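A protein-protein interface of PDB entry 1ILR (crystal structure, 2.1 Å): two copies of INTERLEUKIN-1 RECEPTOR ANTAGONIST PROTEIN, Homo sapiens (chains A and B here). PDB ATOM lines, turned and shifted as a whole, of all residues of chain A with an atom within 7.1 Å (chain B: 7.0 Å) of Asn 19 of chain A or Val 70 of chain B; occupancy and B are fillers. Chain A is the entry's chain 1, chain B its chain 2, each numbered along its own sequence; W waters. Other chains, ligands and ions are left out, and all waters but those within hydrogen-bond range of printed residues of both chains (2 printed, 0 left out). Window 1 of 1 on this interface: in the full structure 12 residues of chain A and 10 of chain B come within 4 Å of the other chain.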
ATOM      1  N   TRP A  16      12.858 -15.733   1.589  1.00  0.00           N
ATOM      2  CA  TRP A  16      12.910 -17.182   1.734  1.00  0.00           C
ATOM      3  C   TRP A  16      14.189 -17.629   1.036  1.00  0.00           C
ATOM      4  O   TRP A  16      14.631 -16.982   0.083  1.00  0.00           O
ATOM      5  CB  TRP A  16      11.640 -17.873   1.179  1.00  0.00           C
ATOM      6  CG  TRP A  16      11.281 -17.656  -0.289  1.00  0.00           C
ATOM      7  CD1 TRP A  16      11.549 -18.503  -1.333  1.00  0.00           C
ATOM      8  CD2 TRP A  16      10.519 -16.570  -0.857  1.00  0.00           C
ATOM      9  NE1 TRP A  16      11.001 -18.019  -2.502  1.00  0.00           N
ATOM     10  CE2 TRP A  16      10.372 -16.833  -2.238  1.00  0.00           C
ATOM     11  CE3 TRP A  16       9.957 -15.404  -0.331  1.00  0.00           C
ATOM     12  CZ2 TRP A  16       9.680 -15.976  -3.095  1.00  0.00           C
ATOM     13  CZ3 TRP A  16       9.269 -14.555  -1.185  1.00  0.00           C
ATOM     14  CH2 TRP A  16       9.141 -14.844  -2.550  1.00  0.00           C
ATOM     15  N   ASP A  17      14.862 -18.655   1.539  1.00  0.00           N
ATOM     16  CA  ASP A  17      16.077 -19.057   0.851  1.00  0.00           C
ATOM     17  C   ASP A  17      15.799 -19.962  -0.339  1.00  0.00           C
ATOM     18  O   ASP A  17      14.670 -20.387  -0.554  1.00  0.00           O
ATOM     19  CB  ASP A  17      17.085 -19.684   1.812  1.00  0.00           C
ATOM     20  CG  ASP A  17      16.584 -20.957   2.441  1.00  0.00           C
ATOM     21  OD1 ASP A  17      15.584 -21.517   1.949  1.00  0.00           O
ATOM     22  OD2 ASP A  17      17.207 -21.402   3.428  1.00  0.00           O
ATOM     23  N   VAL A  18      16.846 -20.296  -1.080  1.00  0.00           N
ATOM     24  CA  VAL A  18      16.721 -21.148  -2.257  1.00  0.00           C
ATOM     25  C   VAL A  18      16.097 -22.516  -1.986  1.00  0.00           C
ATOM     26  O   VAL A  18      15.704 -23.206  -2.932  1.00  0.00           O
ATOM     27  CB  VAL A  18      18.090 -21.361  -2.962  1.00  0.00           C
ATOM     28  CG1 VAL A  18      18.571 -20.065  -3.589  1.00  0.00           C
ATOM     29  CG2 VAL A  18      19.117 -21.885  -1.988  1.00  0.00           C
ATOM     30  N   ASN A  19      16.029 -22.915  -0.715  1.00  0.00           N
ATOM     31  CA  ASN A  19      15.447 -24.199  -0.343  1.00  0.00           C
ATOM     32  C   ASN A  19      14.043 -24.006   0.225  1.00  0.00           C
ATOM     33  O   ASN A  19      13.472 -24.910   0.830  1.00  0.00           O
ATOM     34  CB  ASN A  19      16.347 -24.936   0.653  1.00  0.00           C
ATOM     35  CG  ASN A  19      17.653 -25.403   0.031  1.00  0.00           C
ATOM     36  OD1 ASN A  19      17.653 -26.009  -1.041  1.00  0.00           O
ATOM     37  ND2 ASN A  19      18.771 -25.116   0.693  1.00  0.00           N
ATOM     38  N   GLN A  20      13.516 -22.800   0.039  1.00  0.00           N
ATOM     39  CA  GLN A  20      12.172 -22.417   0.461  1.00  0.00           C
ATOM     40  C   GLN A  20      11.928 -22.171   1.946  1.00  0.00           C
ATOM     41  O   GLN A  20      10.783 -22.055   2.368  1.00  0.00           O
ATOM     42  CB  GLN A  20      11.136 -23.413  -0.084  1.00  0.00           C
ATOM     43  CG  GLN A  20      11.196 -23.672  -1.598  1.00  0.00           C
ATOM     44  CD  GLN A  20      11.062 -22.412  -2.432  1.00  0.00           C
ATOM     45  OE1 GLN A  20      10.301 -21.507  -2.097  1.00  0.00           O
ATOM     46  NE2 GLN A  20      11.805 -22.348  -3.530  1.00  0.00           N
ATOM     47  N   LYS A  21      12.982 -22.095   2.748  1.00  0.00           N
ATOM     48  CA  LYS A  21      12.824 -21.846   4.183  1.00  0.00           C
ATOM     49  C   LYS A  21      12.460 -20.391   4.449  1.00  0.00           C
ATOM     50  O   LYS A  21      12.932 -19.489   3.751  1.00  0.00           O
ATOM     51  CB  LYS A  21      14.114 -22.168   4.958  1.00  0.00           C
ATOM     52  CG  LYS A  21      14.519 -23.642   4.984  1.00  0.00           C
ATOM     53  CD  LYS A  21      15.729 -23.880   5.880  1.00  0.00           C
ATOM     54  CE  LYS A  21      16.082 -25.362   5.966  1.00  0.00           C
ATOM     55  NZ  LYS A  21      16.478 -25.940   4.639  1.00  0.00           N
ATOM     56  N   THR A  22      11.625 -20.179   5.465  1.00  0.00           N
ATOM     57  CA  THR A  22      11.201 -18.841   5.879  1.00  0.00           C
ATOM     58  C   THR A  22      11.813 -18.555   7.240  1.00  0.00           C
ATOM     59  O   THR A  22      12.296 -19.457   7.931  1.00  0.00           O
ATOM     60  CB  THR A  22       9.663 -18.729   6.008  1.00  0.00           C
ATOM     61  OG1 THR A  22       9.162 -19.819   6.788  1.00  0.00           O
ATOM     62  CG2 THR A  22       9.004 -18.762   4.656  1.00  0.00           C
ATOM     63  N   TYR A  34      10.353 -24.457   7.722  1.00  0.00           N
ATOM     64  CA  TYR A  34       9.163 -24.593   6.897  1.00  0.00           C
ATOM     65  C   TYR A  34       7.938 -24.433   7.769  1.00  0.00           C
ATOM     66  O   TYR A  34       7.728 -25.209   8.695  1.00  0.00           O
ATOM     67  CB  TYR A  34       9.152 -25.966   6.231  1.00  0.00           C
ATOM     68  CG  TYR A  34      10.381 -26.204   5.398  1.00  0.00           C
ATOM     69  CD1 TYR A  34      10.531 -25.579   4.166  1.00  0.00           C
ATOM     70  CD2 TYR A  34      11.419 -27.013   5.860  1.00  0.00           C
ATOM     71  CE1 TYR A  34      11.678 -25.739   3.416  1.00  0.00           C
ATOM     72  CE2 TYR A  34      12.574 -27.183   5.116  1.00  0.00           C
ATOM     73  CZ  TYR A  34      12.695 -26.539   3.891  1.00  0.00           C
ATOM     74  OH  TYR A  34      13.839 -26.671   3.136  1.00  0.00           O
ATOM     75  N   THR A 123      21.694 -19.325   6.006  1.00  0.00           N
ATOM     76  CA  THR A 123      20.861 -20.275   6.733  1.00  0.00           C
ATOM     77  C   THR A 123      21.496 -21.659   6.566  1.00  0.00           C
ATOM     78  O   THR A 123      22.364 -21.852   5.713  1.00  0.00           O
ATOM     79  CB  THR A 123      19.400 -20.310   6.199  1.00  0.00           C
ATOM     80  OG1 THR A 123      19.413 -20.444   4.776  1.00  0.00           O
ATOM     81  CG2 THR A 123      18.652 -19.037   6.572  1.00  0.00           C
ATOM     82  N   ALA A 124      21.109 -22.597   7.419  1.00  0.00           N
ATOM     83  CA  ALA A 124      21.625 -23.950   7.345  1.00  0.00           C
ATOM     84  C   ALA A 124      20.751 -24.751   6.389  1.00  0.00           C
ATOM     85  O   ALA A 124      19.616 -24.358   6.087  1.00  0.00           O
ATOM     86  CB  ALA A 124      21.607 -24.587   8.722  1.00  0.00           C
ATOM     87  N   MET A 125      21.288 -25.855   5.879  1.00  0.00           N
ATOM     88  CA  MET A 125      20.516 -26.709   4.988  1.00  0.00           C
ATOM     89  C   MET A 125      19.476 -27.477   5.806  1.00  0.00           C
ATOM     90  O   MET A 125      18.378 -27.749   5.316  1.00  0.00           O
ATOM     91  CB  MET A 125      21.420 -27.655   4.191  1.00  0.00           C
ATOM     92  CG  MET A 125      22.160 -26.952   3.051  1.00  0.00           C
ATOM     93  SD  MET A 125      23.056 -28.029   1.911  1.00  0.00           S
ATOM     94  CE  MET A 125      24.563 -28.319   2.865  1.00  0.00           C
ATOM     95  N   GLU A 126      19.806 -27.792   7.059  1.00  0.00           N
ATOM     96  CA  GLU A 126      18.879 -28.499   7.932  1.00  0.00           C
ATOM     97  C   GLU A 126      17.911 -27.454   8.469  1.00  0.00           C
ATOM     98  O   GLU A 126      18.290 -26.295   8.640  1.00  0.00           O
ATOM     99  CB  GLU A 126      19.609 -29.158   9.106  1.00  0.00           C
ATOM    100  CG  GLU A 126      20.832 -29.994   8.731  1.00  0.00           C
ATOM    101  CD  GLU A 126      22.085 -29.145   8.517  1.00  0.00           C
ATOM    102  OE1 GLU A 126      22.439 -28.356   9.423  1.00  0.00           O
ATOM    103  OE2 GLU A 126      22.716 -29.261   7.444  1.00  0.00           O
ATOM    104  N   VAL A 143      23.533 -21.756   3.206  1.00  0.00           N
ATOM    105  CA  VAL A 143      22.853 -21.131   2.075  1.00  0.00           C
ATOM    106  C   VAL A 143      22.974 -19.602   2.180  1.00  0.00           C
ATOM    107  O   VAL A 143      22.763 -19.033   3.252  1.00  0.00           O
ATOM    108  CB  VAL A 143      21.369 -21.560   2.030  1.00  0.00           C
ATOM    109  CG1 VAL A 143      20.661 -20.925   0.852  1.00  0.00           C
ATOM    110  CG2 VAL A 143      21.280 -23.076   1.948  1.00  0.00           C
ATOM    111  N   LYS A 145      21.876 -17.485  -0.710  1.00  0.00           N
ATOM    112  CA  LYS A 145      21.060 -16.885  -1.753  1.00  0.00           C
ATOM    113  C   LYS A 145      19.642 -16.912  -1.236  1.00  0.00           C
ATOM    114  O   LYS A 145      19.224 -17.900  -0.621  1.00  0.00           O
ATOM    115  CB  LYS A 145      21.149 -17.688  -3.046  1.00  0.00           C
ATOM    116  CG  LYS A 145      22.547 -17.766  -3.625  1.00  0.00           C
ATOM    117  CD  LYS A 145      23.076 -16.395  -3.996  1.00  0.00           C
ATOM    118  CE  LYS A 145      24.556 -16.471  -4.323  1.00  0.00           C
ATOM    119  NZ  LYS A 145      25.061 -15.149  -4.759  1.00  0.00           N
ATOM    120  N   TYR A 147      15.382 -15.305  -1.977  1.00  0.00           N
ATOM    121  CA  TYR A 147      14.444 -14.654  -2.869  1.00  0.00           C
ATOM    122  C   TYR A 147      13.958 -13.540  -1.957  1.00  0.00           C
ATOM    123  O   TYR A 147      13.476 -13.789  -0.849  1.00  0.00           O
ATOM    124  CB  TYR A 147      13.329 -15.608  -3.270  1.00  0.00           C
ATOM    125  CG  TYR A 147      13.842 -16.729  -4.140  1.00  0.00           C
ATOM    126  CD1 TYR A 147      14.381 -17.884  -3.578  1.00  0.00           C
ATOM    127  CD2 TYR A 147      13.844 -16.608  -5.525  1.00  0.00           C
ATOM    128  CE1 TYR A 147      14.906 -18.884  -4.370  1.00  0.00           C
ATOM    129  CE2 TYR A 147      14.371 -17.609  -6.331  1.00  0.00           C
ATOM    130  CZ  TYR A 147      14.903 -18.743  -5.748  1.00  0.00           C
ATOM    131  OH  TYR A 147      15.437 -19.742  -6.545  1.00  0.00           O
ATOM    132  N   SER B  68      14.817 -35.920   0.234  1.00  0.00           N
ATOM    133  CA  SER B  68      14.698 -34.607  -0.370  1.00  0.00           C
ATOM    134  C   SER B  68      16.057 -34.077  -0.757  1.00  0.00           C
ATOM    135  O   SER B  68      17.070 -34.536  -0.233  1.00  0.00           O
ATOM    136  CB  SER B  68      14.051 -33.653   0.626  1.00  0.00           C
ATOM    137  OG  SER B  68      14.790 -33.625   1.837  1.00  0.00           O
ATOM    138  N   CYS B  69      16.084 -33.119  -1.676  1.00  0.00           N
ATOM    139  CA  CYS B  69      17.339 -32.500  -2.087  1.00  0.00           C
ATOM    140  C   CYS B  69      17.364 -31.054  -1.610  1.00  0.00           C
ATOM    141  O   CYS B  69      16.396 -30.308  -1.794  1.00  0.00           O
ATOM    142  CB  CYS B  69      17.524 -32.522  -3.611  1.00  0.00           C
ATOM    143  SG  CYS B  69      19.021 -31.623  -4.182  1.00  0.00           S
ATOM    144  N   VAL B  70      18.420 -30.694  -0.896  1.00  0.00           N
ATOM    145  CA  VAL B  70      18.590 -29.312  -0.445  1.00  0.00           C
ATOM    146  C   VAL B  70      19.928 -28.856  -1.030  1.00  0.00           C
ATOM    147  O   VAL B  70      20.893 -29.631  -1.063  1.00  0.00           O
ATOM    148  CB  VAL B  70      18.548 -29.147   1.111  1.00  0.00           C
ATOM    149  CG1 VAL B  70      17.129 -29.359   1.610  1.00  0.00           C
ATOM    150  CG2 VAL B  70      19.521 -30.108   1.786  1.00  0.00           C
ATOM    151  N   LYS B  71      19.955 -27.649  -1.577  1.00  0.00           N
ATOM    152  CA  LYS B  71      21.170 -27.144  -2.168  1.00  0.00           C
ATOM    153  C   LYS B  71      21.816 -26.000  -1.419  1.00  0.00           C
ATOM    154  O   LYS B  71      21.266 -25.482  -0.436  1.00  0.00           O
ATOM    155  CB  LYS B  71      20.936 -26.751  -3.629  1.00  0.00           C
ATOM    156  CG  LYS B  71      19.662 -25.988  -3.870  1.00  0.00           C
ATOM    157  CD  LYS B  71      19.409 -25.894  -5.349  1.00  0.00           C
ATOM    158  CE  LYS B  71      17.948 -25.644  -5.642  1.00  0.00           C
ATOM    159  NZ  LYS B  71      17.734 -25.632  -7.113  1.00  0.00           N
ATOM    160  N   SER B  72      23.015 -25.659  -1.882  1.00  0.00           N
ATOM    161  CA  SER B  72      23.832 -24.593  -1.331  1.00  0.00           C
ATOM    162  C   SER B  72      24.799 -24.191  -2.452  1.00  0.00           C
ATOM    163  O   SER B  72      25.949 -24.620  -2.490  1.00  0.00           O
ATOM    164  CB  SER B  72      24.598 -25.078  -0.112  1.00  0.00           C
ATOM    165  OG  SER B  72      25.355 -24.023   0.445  1.00  0.00           O
ATOM    166  N   GLU B  75      26.338 -27.140  -4.966  1.00  0.00           N
ATOM    167  CA  GLU B  75      26.379 -28.414  -4.272  1.00  0.00           C
ATOM    168  C   GLU B  75      24.993 -28.747  -3.758  1.00  0.00           C
ATOM    169  O   GLU B  75      24.224 -27.856  -3.402  1.00  0.00           O
ATOM    170  CB  GLU B  75      27.374 -28.371  -3.117  1.00  0.00           C
ATOM    171  CG  GLU B  75      28.812 -28.252  -3.576  1.00  0.00           C
ATOM    172  CD  GLU B  75      29.810 -28.510  -2.470  1.00  0.00           C
ATOM    173  OE1 GLU B  75      29.524 -29.353  -1.588  1.00  0.00           O
ATOM    174  OE2 GLU B  75      30.887 -27.875  -2.496  1.00  0.00           O
ATOM    175  N   THR B  76      24.668 -30.032  -3.753  1.00  0.00           N
ATOM    176  CA  THR B  76      23.372 -30.504  -3.287  1.00  0.00           C
ATOM    177  C   THR B  76      23.581 -31.527  -2.177  1.00  0.00           C
ATOM    178  O   THR B  76      24.691 -32.025  -1.979  1.00  0.00           O
ATOM    179  CB  THR B  76      22.595 -31.179  -4.424  1.00  0.00           C
ATOM    180  OG1 THR B  76      23.424 -32.181  -5.023  1.00  0.00           O
ATOM    181  CG2 THR B  76      22.181 -30.165  -5.478  1.00  0.00           C
ATOM    182  N   ARG B  77      22.510 -31.851  -1.465  1.00  0.00           N
ATOM    183  CA  ARG B  77      22.581 -32.816  -0.387  1.00  0.00           C
ATOM    184  C   ARG B  77      21.290 -33.630  -0.339  1.00  0.00           C
ATOM    185  O   ARG B  77      20.204 -33.108  -0.620  1.00  0.00           O
ATOM    186  CB  ARG B  77      22.814 -32.086   0.934  1.00  0.00           C
ATOM    187  CG  ARG B  77      22.821 -32.981   2.134  1.00  0.00           C
ATOM    188  CD  ARG B  77      22.885 -32.182   3.419  1.00  0.00           C
ATOM    189  NE  ARG B  77      22.616 -33.044   4.566  1.00  0.00           N
ATOM    190  CZ  ARG B  77      22.834 -32.708   5.832  1.00  0.00           C
ATOM    191  NH1 ARG B  77      23.331 -31.517   6.125  1.00  0.00           N
ATOM    192  NH2 ARG B  77      22.561 -33.573   6.803  1.00  0.00           N
ATOM    193  N   LEU B  78      21.428 -34.920  -0.034  1.00  0.00           N
ATOM    194  CA  LEU B  78      20.288 -35.823   0.067  1.00  0.00           C
ATOM    195  C   LEU B  78      19.919 -35.980   1.531  1.00  0.00           C
ATOM    196  O   LEU B  78      20.736 -36.400   2.335  1.00  0.00           O
ATOM    197  CB  LEU B  78      20.623 -37.197  -0.513  1.00  0.00           C
ATOM    198  CG  LEU B  78      19.440 -38.174  -0.535  1.00  0.00           C
ATOM    199  CD1 LEU B  78      18.473 -37.796  -1.637  1.00  0.00           C
ATOM    200  CD2 LEU B  78      19.917 -39.586  -0.732  1.00  0.00           C
ATOM    201  N   GLN B  79      18.684 -35.658   1.877  1.00  0.00           N
ATOM    202  CA  GLN B  79      18.239 -35.781   3.253  1.00  0.00           C
ATOM    203  C   GLN B  79      17.020 -36.688   3.394  1.00  0.00           C
ATOM    204  O   GLN B  79      16.224 -36.852   2.460  1.00  0.00           O
ATOM    205  CB  GLN B  79      17.866 -34.413   3.828  1.00  0.00           C
ATOM    206  CG  GLN B  79      18.908 -33.338   3.676  1.00  0.00           C
ATOM    207  CD  GLN B  79      18.487 -32.038   4.334  1.00  0.00           C
ATOM    208  OE1 GLN B  79      19.232 -31.470   5.139  1.00  0.00           O
ATOM    209  NE2 GLN B  79      17.286 -31.557   3.996  1.00  0.00           N
ATOM    210  N   GLU B  81      13.919 -36.765   5.746  1.00  0.00           N
ATOM    211  CA  GLU B  81      13.227 -35.968   6.733  1.00  0.00           C
ATOM    212  C   GLU B  81      12.064 -36.741   7.324  1.00  0.00           C
ATOM    213  O   GLU B  81      11.426 -37.525   6.636  1.00  0.00           O
ATOM    214  CB  GLU B  81      12.757 -34.670   6.096  1.00  0.00           C
ATOM    215  CG  GLU B  81      13.860 -33.980   5.312  1.00  0.00           C
ATOM    216  CD  GLU B  81      13.498 -32.573   4.862  1.00  0.00           C
ATOM    217  OE1 GLU B  81      12.556 -31.979   5.429  1.00  0.00           O
ATOM    218  OE2 GLU B  81      14.173 -32.045   3.953  1.00  0.00           O
ATOM    219  N   LYS B  93       4.802 -24.984  -2.698  1.00  0.00           N
ATOM    220  CA  LYS B  93       6.143 -24.479  -2.934  1.00  0.00           C
ATOM    221  C   LYS B  93       7.246 -25.225  -2.196  1.00  0.00           C
ATOM    222  O   LYS B  93       8.146 -25.796  -2.814  1.00  0.00           O
ATOM    223  CB  LYS B  93       6.153 -23.013  -2.510  1.00  0.00           C
ATOM    224  CG  LYS B  93       7.212 -22.139  -3.117  1.00  0.00           C
ATOM    225  CD  LYS B  93       7.088 -20.754  -2.495  1.00  0.00           C
ATOM    226  CE  LYS B  93       8.048 -19.750  -3.103  1.00  0.00           C
ATOM    227  NZ  LYS B  93       7.827 -18.404  -2.499  1.00  0.00           N
ATOM    228  N   GLN B  94       7.154 -25.220  -0.869  1.00  0.00           N
ATOM    229  CA  GLN B  94       8.151 -25.850  -0.006  1.00  0.00           C
ATOM    230  C   GLN B  94       8.324 -27.360  -0.118  1.00  0.00           C
ATOM    231  O   GLN B  94       9.389 -27.885   0.210  1.00  0.00           O
ATOM    232  CB  GLN B  94       7.913 -25.468   1.464  1.00  0.00           C
ATOM    233  CG  GLN B  94       6.581 -25.921   2.042  1.00  0.00           C
ATOM    234  CD  GLN B  94       6.392 -25.493   3.489  1.00  0.00           C
ATOM    235  OE1 GLN B  94       6.645 -26.267   4.422  1.00  0.00           O
ATOM    236  NE2 GLN B  94       5.927 -24.264   3.685  1.00  0.00           N
ATOM    237  N   ARG B  97      11.080 -29.943  -2.727  1.00  0.00           N
ATOM    238  CA  ARG B  97      12.353 -30.588  -2.394  1.00  0.00           C
ATOM    239  C   ARG B  97      12.237 -32.108  -2.253  1.00  0.00           C
ATOM    240  O   ARG B  97      13.240 -32.817  -2.243  1.00  0.00           O
ATOM    241  CB  ARG B  97      12.931 -29.986  -1.109  1.00  0.00           C
ATOM    242  CG  ARG B  97      12.130 -30.271   0.155  1.00  0.00           C
ATOM    243  CD  ARG B  97      12.703 -29.490   1.306  1.00  0.00           C
ATOM    244  NE  ARG B  97      12.167 -29.897   2.601  1.00  0.00           N
ATOM    245  CZ  ARG B  97      11.015 -29.473   3.109  1.00  0.00           C
ATOM    246  NH1 ARG B  97      10.245 -28.630   2.433  1.00  0.00           N
ATOM    247  NH2 ARG B  97      10.680 -29.828   4.340  1.00  0.00           N
ATOM    248  N   SER B 113      16.082 -35.271  -9.148  1.00  0.00           N
ATOM    249  CA  SER B 113      15.543 -34.271  -8.229  1.00  0.00           C
ATOM    250  C   SER B 113      14.839 -33.154  -8.968  1.00  0.00           C
ATOM    251  O   SER B 113      15.400 -32.539  -9.872  1.00  0.00           O
ATOM    252  CB  SER B 113      16.655 -33.655  -7.377  1.00  0.00           C
ATOM    253  OG  SER B 113      16.135 -32.697  -6.463  1.00  0.00           O
ATOM    254  N   ALA B 115      13.705 -30.479  -7.319  1.00  0.00           N
ATOM    255  CA  ALA B 115      14.203 -29.265  -6.676  1.00  0.00           C
ATOM    256  C   ALA B 115      15.624 -28.930  -7.102  1.00  0.00           C
ATOM    257  O   ALA B 115      16.032 -27.770  -7.046  1.00  0.00           O
ATOM    258  CB  ALA B 115      14.126 -29.389  -5.168  1.00  0.00           C
ATOM    259  N   CYS B 116      16.369 -29.945  -7.532  1.00  0.00           N
ATOM    260  CA  CYS B 116      17.753 -29.779  -7.980  1.00  0.00           C
ATOM    261  C   CYS B 116      17.917 -30.493  -9.331  1.00  0.00           C
ATOM    262  O   CYS B 116      18.597 -31.517  -9.425  1.00  0.00           O
ATOM    263  CB  CYS B 116      18.710 -30.396  -6.954  1.00  0.00           C
ATOM    264  SG  CYS B 116      18.320 -30.024  -5.219  1.00  0.00           S
ATOM    265  N   LEU B 133      23.376 -37.961  -4.455  1.00  0.00           N
ATOM    266  CA  LEU B 133      22.884 -37.373  -5.695  1.00  0.00           C
ATOM    267  C   LEU B 133      24.075 -37.000  -6.569  1.00  0.00           C
ATOM    268  O   LEU B 133      25.099 -36.571  -6.052  1.00  0.00           O
ATOM    269  CB  LEU B 133      22.083 -36.109  -5.387  1.00  0.00           C
ATOM    270  CG  LEU B 133      20.725 -36.260  -4.703  1.00  0.00           C
ATOM    271  CD1 LEU B 133      20.390 -34.981  -3.977  1.00  0.00           C
ATOM    272  CD2 LEU B 133      19.651 -36.612  -5.729  1.00  0.00           C
HETATM  273  O   HOH W   1      16.119 -29.225   5.309  1.00  0.00           O
HETATM  274  O   HOH W   2      15.437 -27.609  -2.285  1.00  0.00           O
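Among the printed residues, merely in contact across the chains: Asn 19 of chain A with Val 70 of chain B (3.5 Å), Gln 20 of chain A with Lys 93 of chain B (3.0 Å), Gln 20 of chain A with Gln 94 of chain B (3.9 Å), Tyr 34 of chain A with Gln 94 of chain B (3.1 Å), Tyr 34 of chain A with Arg 97 of chain B (3.3 Å), Met 125 of chain A with Val 70 of chain B (3.9 Å), Met 125 of chain A with Lys 71 of chain B (3.9 Å), Met 125 of chain A with Ser 72 of chain B (3.9 Å), Met 125 of chain A with Gln 79 of chain B (3.8 Å) and Val 143 of chain A with Lys 71 of chain B (3.4 Å).
The backbone carbonyl oxygen (O) of Lys 71 of chain B lies within hydrogen-bond range of the side-chain amide nitrogen (ND2) of Asn 19 of chain A.
The guanidinium group (NH1) of Arg 77 of chain B is in salt-bridge range of the side-chain carboxylate (OE2) of Glu 126 of chain A (2.7 Å).
NE1 of Trp 16 of chain A lies close to NZ of Lys 93 of chain B (3.2 Å).
Water W1 lies within hydrogen-bond range of the backbone carbonyl oxygen (O) of Met 125 of chain A, the side-chain amide nitrogen (NE2) of Gln 79 of chain B and the side-chain amino group (NZ) of Lys 21 of chain A.
Water W2 lies within hydrogen-bond range of the backbone carbonyl oxygen (O) of Cys 69 of chain B (2.9 Å) and the side-chain amide oxygen (OD1) of Asn 19 of chain A (3.0 Å).
No position is printed for both chains.
Of the 13 pairs that touch across the chains among the printed residues, none has its exchanged pair printed and touching as well.
O of Asn 19 of chain A is in hydrogen-bond range of OH of Tyr 34 of chain A, at 2.9 Å.
NZ of Lys 21 of chain A lies within hydrogen-bond range of O of Met 125 of chain A (2.7 Å).
N of Cys 69 of chain B sits at hydrogen-bond distance from O of Arg 97 of chain B (2.9 Å).
O of Val 70 of chain B sits at hydrogen-bond distance from N of Arg 77 of chain B (2.8 Å).
The side-chain amide nitrogen (NE2) of Gln 79 of chain B sits at hydrogen-bond distance from the side-chain carboxylate (OE2) of Glu 81 of chain B, at 3.2 Å.
SG of Cys 69 of chain B is disulfide-bonded to SG of Cys 116 of chain B.
Of the 18 printed residues of chain B, 8 touch a printed residue of chain A.
Of the 15 printed residues of chain A, 7 touch a printed residue of chain B.
Printed residues of chain A that touch a printed residue of chain B: Trp 16, Asn 19, Gln 20, Tyr 34, Met 125, Glu 126 and Val 143.
Hydrophobic or aromatic side chains of chain A that line the printed part of chain B: Trp 16, Tyr 34, Met 125 and Val 143.
Among the printed residues, Asp or Glu carboxylates within 4 Å of a Lys or Arg side-chain nitrogen of the other chain: Glu 126 of chain A with Arg 77 of chain B (2.7 Å).
Of the printed residues of chain B, Tyr 34 of chain A touches Gln 94 and Arg 97.
Val 70 of chain B touches just these residues of chain A: Asn 19 and Met 125.
Of the printed residues of chain A, Arg 97 of chain B touches Tyr 34.
Cys 116 of chain B touches none of the printed residues of chain A.
The nearest residue of chain A that does not touch Val 70 of chain B is Tyr 34 of chain A (4.5 Å).
The nearest printed residue of chain B that does not touch Gln 20 of chain A is Arg 97 of chain B (5.9 Å).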
